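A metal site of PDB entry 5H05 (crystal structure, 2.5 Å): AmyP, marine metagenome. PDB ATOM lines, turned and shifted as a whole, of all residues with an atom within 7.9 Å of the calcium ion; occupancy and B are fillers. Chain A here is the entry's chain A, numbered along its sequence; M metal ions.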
ATOM      1  N   GLU A  22      16.796   7.654 -30.494  1.00  0.00           N
ATOM      2  CA  GLU A  22      16.471   7.816 -29.084  1.00  0.00           C
ATOM      3  C   GLU A  22      17.710   7.949 -28.214  1.00  0.00           C
ATOM      4  O   GLU A  22      17.675   8.655 -27.207  1.00  0.00           O
ATOM      5  CB  GLU A  22      15.587   6.671 -28.558  1.00  0.00           C
ATOM      6  CG  GLU A  22      16.183   5.245 -28.662  1.00  0.00           C
ATOM      7  CD  GLU A  22      16.847   4.720 -27.377  1.00  0.00           C
ATOM      8  OE1 GLU A  22      16.702   5.331 -26.294  1.00  0.00           O
ATOM      9  OE2 GLU A  22      17.516   3.664 -27.446  1.00  0.00           O
ATOM     10  N   VAL A  25      21.700  12.270 -29.376  1.00  0.00           N
ATOM     11  CA  VAL A  25      21.863  13.542 -28.669  1.00  0.00           C
ATOM     12  C   VAL A  25      20.495  14.038 -28.196  1.00  0.00           C
ATOM     13  O   VAL A  25      19.584  14.231 -29.005  1.00  0.00           O
ATOM     14  CB  VAL A  25      22.531  14.601 -29.554  1.00  0.00           C
ATOM     15  CG1 VAL A  25      22.539  15.942 -28.839  1.00  0.00           C
ATOM     16  CG2 VAL A  25      23.935  14.183 -29.902  1.00  0.00           C
ATOM     17  N   ASN A  26      20.377  14.238 -26.884  1.00  0.00           N
ATOM     18  CA  ASN A  26      19.217  14.921 -26.310  1.00  0.00           C
ATOM     19  C   ASN A  26      19.391  16.420 -26.553  1.00  0.00           C
ATOM     20  O   ASN A  26      20.009  17.126 -25.760  1.00  0.00           O
ATOM     21  CB  ASN A  26      19.071  14.583 -24.830  1.00  0.00           C
ATOM     22  CG  ASN A  26      18.014  15.458 -24.131  1.00  0.00           C
ATOM     23  OD1 ASN A  26      17.298  16.216 -24.771  1.00  0.00           O
ATOM     24  ND2 ASN A  26      17.912  15.333 -22.812  1.00  0.00           N
ATOM     25  N   GLY A  27      18.813  16.910 -27.660  1.00  0.00           N
ATOM     26  CA  GLY A  27      18.989  18.286 -28.065  1.00  0.00           C
ATOM     27  C   GLY A  27      17.919  19.238 -27.562  1.00  0.00           C
ATOM     28  O   GLY A  27      18.121  20.450 -27.559  1.00  0.00           O
ATOM     29  N   ASP A  28      16.758  18.707 -27.158  1.00  0.00           N
ATOM     30  CA  ASP A  28      15.629  19.506 -26.675  1.00  0.00           C
ATOM     31  C   ASP A  28      15.155  18.846 -25.391  1.00  0.00           C
ATOM     32  O   ASP A  28      14.317  17.945 -25.427  1.00  0.00           O
ATOM     33  CB  ASP A  28      14.529  19.595 -27.726  1.00  0.00           C
ATOM     34  CG  ASP A  28      13.282  20.337 -27.239  1.00  0.00           C
ATOM     35  OD1 ASP A  28      13.321  20.945 -26.149  1.00  0.00           O
ATOM     36  OD2 ASP A  28      12.260  20.315 -27.967  1.00  0.00           O
ATOM     37  N   ASP A  29      15.660  19.309 -24.253  1.00  0.00           N
ATOM     38  CA  ASP A  29      15.418  18.524 -23.051  1.00  0.00           C
ATOM     39  C   ASP A  29      13.954  18.500 -22.655  1.00  0.00           C
ATOM     40  O   ASP A  29      13.618  17.850 -21.656  1.00  0.00           O
ATOM     41  CB  ASP A  29      16.272  19.033 -21.891  1.00  0.00           C
ATOM     42  CG  ASP A  29      16.352  18.028 -20.764  1.00  0.00           C
ATOM     43  OD1 ASP A  29      17.098  17.028 -20.897  1.00  0.00           O
ATOM     44  OD2 ASP A  29      15.663  18.223 -19.730  1.00  0.00           O
ATOM     45  N   ALA A  30      13.077  19.162 -23.396  1.00  0.00           N
ATOM     46  CA  ALA A  30      11.665  19.159 -23.087  1.00  0.00           C
ATOM     47  C   ALA A  30      10.924  17.971 -23.688  1.00  0.00           C
ATOM     48  O   ALA A  30       9.765  17.742 -23.321  1.00  0.00           O
ATOM     49  CB  ALA A  30      11.012  20.447 -23.599  1.00  0.00           C
ATOM     50  N   ILE A  31      11.534  17.221 -24.602  1.00  0.00           N
ATOM     51  CA  ILE A  31      10.854  16.128 -25.277  1.00  0.00           C
ATOM     52  C   ILE A  31      11.724  14.881 -25.207  1.00  0.00           C
ATOM     53  O   ILE A  31      12.946  14.957 -25.043  1.00  0.00           O
ATOM     54  CB  ILE A  31      10.497  16.458 -26.750  1.00  0.00           C
ATOM     55  CG1 ILE A  31      11.750  16.600 -27.601  1.00  0.00           C
ATOM     56  CG2 ILE A  31       9.720  17.751 -26.831  1.00  0.00           C
ATOM     57  CD1 ILE A  31      11.442  16.821 -29.065  1.00  0.00           C
ATOM     58  N   GLY A  32      11.079  13.737 -25.337  1.00  0.00           N
ATOM     59  CA  GLY A  32      11.794  12.477 -25.458  1.00  0.00           C
ATOM     60  C   GLY A  32      11.081  11.348 -24.748  1.00  0.00           C
ATOM     61  O   GLY A  32      10.260  11.559 -23.860  1.00  0.00           O
ATOM     62  N   HIS A  33      11.417  10.117 -25.149  1.00  0.00           N
ATOM     63  CA  HIS A  33      10.756   8.944 -24.595  1.00  0.00           C
ATOM     64  C   HIS A  33      11.105   8.750 -23.122  1.00  0.00           C
ATOM     65  O   HIS A  33      10.254   8.381 -22.300  1.00  0.00           O
ATOM     66  CB  HIS A  33      11.127   7.709 -25.395  1.00  0.00           C
ATOM     67  CG  HIS A  33      10.570   7.688 -26.781  1.00  0.00           C
ATOM     68  ND1 HIS A  33       9.295   7.244 -27.063  1.00  0.00           N
ATOM     69  CD2 HIS A  33      11.115   8.043 -27.964  1.00  0.00           C
ATOM     70  CE1 HIS A  33       9.083   7.334 -28.371  1.00  0.00           C
ATOM     71  NE2 HIS A  33      10.172   7.809 -28.932  1.00  0.00           N
ATOM     72  N   HIS A  41      20.345   8.065 -22.264  1.00  0.00           N
ATOM     73  CA  HIS A  41      19.364   8.985 -21.705  1.00  0.00           C
ATOM     74  C   HIS A  41      17.953   8.764 -22.256  1.00  0.00           C
ATOM     75  O   HIS A  41      16.996   9.251 -21.642  1.00  0.00           O
ATOM     76  CB  HIS A  41      19.820  10.412 -21.972  1.00  0.00           C
ATOM     77  CG  HIS A  41      20.297  10.668 -23.374  1.00  0.00           C
ATOM     78  ND1 HIS A  41      19.437  10.757 -24.455  1.00  0.00           N
ATOM     79  CD2 HIS A  41      21.537  10.864 -23.878  1.00  0.00           C
ATOM     80  CE1 HIS A  41      20.131  10.992 -25.554  1.00  0.00           C
ATOM     81  NE2 HIS A  41      21.412  11.063 -25.231  1.00  0.00           N
ATOM     82  N   HIS A  42      17.793   8.073 -23.378  1.00  0.00           N
ATOM     83  CA  HIS A  42      16.480   7.798 -23.997  1.00  0.00           C
ATOM     84  C   HIS A  42      15.722   9.077 -24.357  1.00  0.00           C
ATOM     85  O   HIS A  42      14.493   9.081 -24.449  1.00  0.00           O
ATOM     86  CB  HIS A  42      15.599   6.900 -23.111  1.00  0.00           C
ATOM     87  CG  HIS A  42      16.239   5.597 -22.745  1.00  0.00           C
ATOM     88  ND1 HIS A  42      16.728   4.710 -23.685  1.00  0.00           N
ATOM     89  CD2 HIS A  42      16.464   5.025 -21.538  1.00  0.00           C
ATOM     90  CE1 HIS A  42      17.225   3.648 -23.070  1.00  0.00           C
ATOM     91  NE2 HIS A  42      17.077   3.816 -21.771  1.00  0.00           N
ATOM     92  N   LYS A  43      16.448  10.155 -24.599  1.00  0.00           N
ATOM     93  CA  LYS A  43      15.821  11.438 -24.910  1.00  0.00           C
ATOM     94  C   LYS A  43      16.415  12.061 -26.157  1.00  0.00           C
ATOM     95  O   LYS A  43      16.299  13.267 -26.345  1.00  0.00           O
ATOM     96  CB  LYS A  43      15.941  12.399 -23.720  1.00  0.00           C
ATOM     97  CG  LYS A  43      15.187  11.925 -22.469  1.00  0.00           C
ATOM     98  CD  LYS A  43      15.280  12.946 -21.320  1.00  0.00           C
ATOM     99  CE  LYS A  43      14.328  14.134 -21.527  1.00  0.00           C
ATOM    100  NZ  LYS A  43      14.407  15.093 -20.397  1.00  0.00           N
ATOM    101  N   GLY A  44      17.062  11.270 -27.011  1.00  0.00           N
ATOM    102  CA  GLY A  44      17.507  11.800 -28.288  1.00  0.00           C
ATOM    103  C   GLY A  44      16.335  12.213 -29.144  1.00  0.00           C
ATOM    104  O   GLY A  44      15.225  11.686 -29.023  1.00  0.00           O
ATOM    105  N   ASP A  45      16.584  13.168 -30.049  1.00  0.00           N
ATOM    106  CA  ASP A  45      15.522  13.834 -30.796  1.00  0.00           C
ATOM    107  C   ASP A  45      16.103  14.460 -32.061  1.00  0.00           C
ATOM    108  O   ASP A  45      17.314  14.384 -32.313  1.00  0.00           O
ATOM    109  CB  ASP A  45      14.848  14.893 -29.925  1.00  0.00           C
ATOM    110  CG  ASP A  45      15.845  15.862 -29.289  1.00  0.00           C
ATOM    111  OD1 ASP A  45      16.859  16.217 -29.931  1.00  0.00           O
ATOM    112  OD2 ASP A  45      15.614  16.278 -28.134  1.00  0.00           O
ATOM    113  N   LEU A  46      15.243  15.108 -32.846  1.00  0.00           N
ATOM    114  CA  LEU A  46      15.713  15.650 -34.118  1.00  0.00           C
ATOM    115  C   LEU A  46      16.579  16.882 -33.916  1.00  0.00           C
ATOM    116  O   LEU A  46      17.433  17.170 -34.757  1.00  0.00           O
ATOM    117  CB  LEU A  46      14.518  15.980 -35.013  1.00  0.00           C
ATOM    118  CG  LEU A  46      13.750  14.737 -35.463  1.00  0.00           C
ATOM    119  CD1 LEU A  46      12.800  15.054 -36.616  1.00  0.00           C
ATOM    120  CD2 LEU A  46      14.725  13.643 -35.858  1.00  0.00           C
ATOM    121  N   GLN A  47      16.378  17.607 -32.824  1.00  0.00           N
ATOM    122  CA  GLN A  47      17.215  18.771 -32.568  1.00  0.00           C
ATOM    123  C   GLN A  47      18.643  18.340 -32.299  1.00  0.00           C
ATOM    124  O   GLN A  47      19.591  18.979 -32.765  1.00  0.00           O
ATOM    125  CB  GLN A  47      16.650  19.580 -31.398  1.00  0.00           C
ATOM    126  CG  GLN A  47      17.325  20.920 -31.183  1.00  0.00           C
ATOM    127  CD  GLN A  47      17.091  21.857 -32.338  1.00  0.00           C
ATOM    128  OE1 GLN A  47      15.952  22.212 -32.627  1.00  0.00           O
ATOM    129  NE2 GLN A  47      18.164  22.245 -33.023  1.00  0.00           N
ATOM    130  N   GLY A  48      18.819  17.225 -31.581  1.00  0.00           N
ATOM    131  CA  GLY A  48      20.156  16.710 -31.332  1.00  0.00           C
ATOM    132  C   GLY A  48      20.891  16.352 -32.599  1.00  0.00           C
ATOM    133  O   GLY A  48      22.062  16.712 -32.778  1.00  0.00           O
ATOM    134  N   ARG A 101       7.800  12.541 -29.604  1.00  0.00           N
ATOM    135  CA  ARG A 101       8.943  12.422 -28.706  1.00  0.00           C
ATOM    136  C   ARG A 101      10.264  12.753 -29.410  1.00  0.00           C
ATOM    137  O   ARG A 101      11.233  13.100 -28.736  1.00  0.00           O
ATOM    138  CB  ARG A 101       9.039  11.033 -28.078  1.00  0.00           C
ATOM    139  CG  ARG A 101       8.247  10.857 -26.789  1.00  0.00           C
ATOM    140  CD  ARG A 101       6.772  10.745 -27.064  1.00  0.00           C
ATOM    141  NE  ARG A 101       6.499   9.733 -28.085  1.00  0.00           N
ATOM    142  CZ  ARG A 101       5.960   8.537 -27.856  1.00  0.00           C
ATOM    143  NH1 ARG A 101       5.766   7.690 -28.865  1.00  0.00           N
ATOM    144  NH2 ARG A 101       5.598   8.207 -26.620  1.00  0.00           N
ATOM    145  N   PHE A 102      10.303  12.662 -30.741  1.00  0.00           N
ATOM    146  CA  PHE A 102      11.485  13.046 -31.505  1.00  0.00           C
ATOM    147  C   PHE A 102      11.440  14.458 -32.053  1.00  0.00           C
ATOM    148  O   PHE A 102      12.495  15.094 -32.196  1.00  0.00           O
ATOM    149  CB  PHE A 102      11.689  12.088 -32.681  1.00  0.00           C
ATOM    150  CG  PHE A 102      11.997  10.697 -32.261  1.00  0.00           C
ATOM    151  CD1 PHE A 102      12.683  10.467 -31.081  1.00  0.00           C
ATOM    152  CD2 PHE A 102      11.581   9.618 -33.026  1.00  0.00           C
ATOM    153  CE1 PHE A 102      12.961   9.176 -30.670  1.00  0.00           C
ATOM    154  CE2 PHE A 102      11.870   8.331 -32.634  1.00  0.00           C
ATOM    155  CZ  PHE A 102      12.561   8.122 -31.449  1.00  0.00           C
HETATM  156 CA    CA M   1      15.339  15.698 -25.880  1.00  0.00          CA
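OD1 of Asp 29 lies within hydrogen-bond range of ND2 of Asn 26 (2.7 Å). OD1 of Asp 45 sits at hydrogen-bond distance from N of Gly 27 (3.1 Å). The backbone carbonyl oxygen (O) of Val 25 is in hydrogen-bond range of the backbone NH (N) of Asp 45. The backbone NH (N) of Gln 47 is in hydrogen-bond range of the side-chain carboxylate (OD1) of Asp 45 (3.2 Å). The side-chain carboxylate of Asp 28 sits close to the backbone NH of Ala 30 (3.3 Å). NZ of Lys 43 lies within salt-bridge range of OD1 of Asp 29, at 3.4 Å. ND1 of His 41 lies within hydrogen-bond range of N of Lys 43, at 3.1 Å. O of Glu 22 sits at hydrogen-bond distance from N of Lys 43, 3.2 Å away.
Residues that only touch the calcium ion: Asp 29 (3.97 Å). Of the 20 residues printed, 6 come within 4 Å of the calcium ion. The nearest printed residue that does not touch the calcium ion is Gly 27 (4.1 Å).
OD1 of Asn 26 is bound to the calcium ion (2.3 Å). OD2 of Asp 45 binds the calcium ion (2.3 Å). O of Asp 28 binds the calcium ion (2.5 Å). O of Ile 31 is bound to the calcium ion (2.6 Å). The calcium ion is bound by O of Lys 43, 2.7 Å away. The calcium ion has five donor atoms within binding distance.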
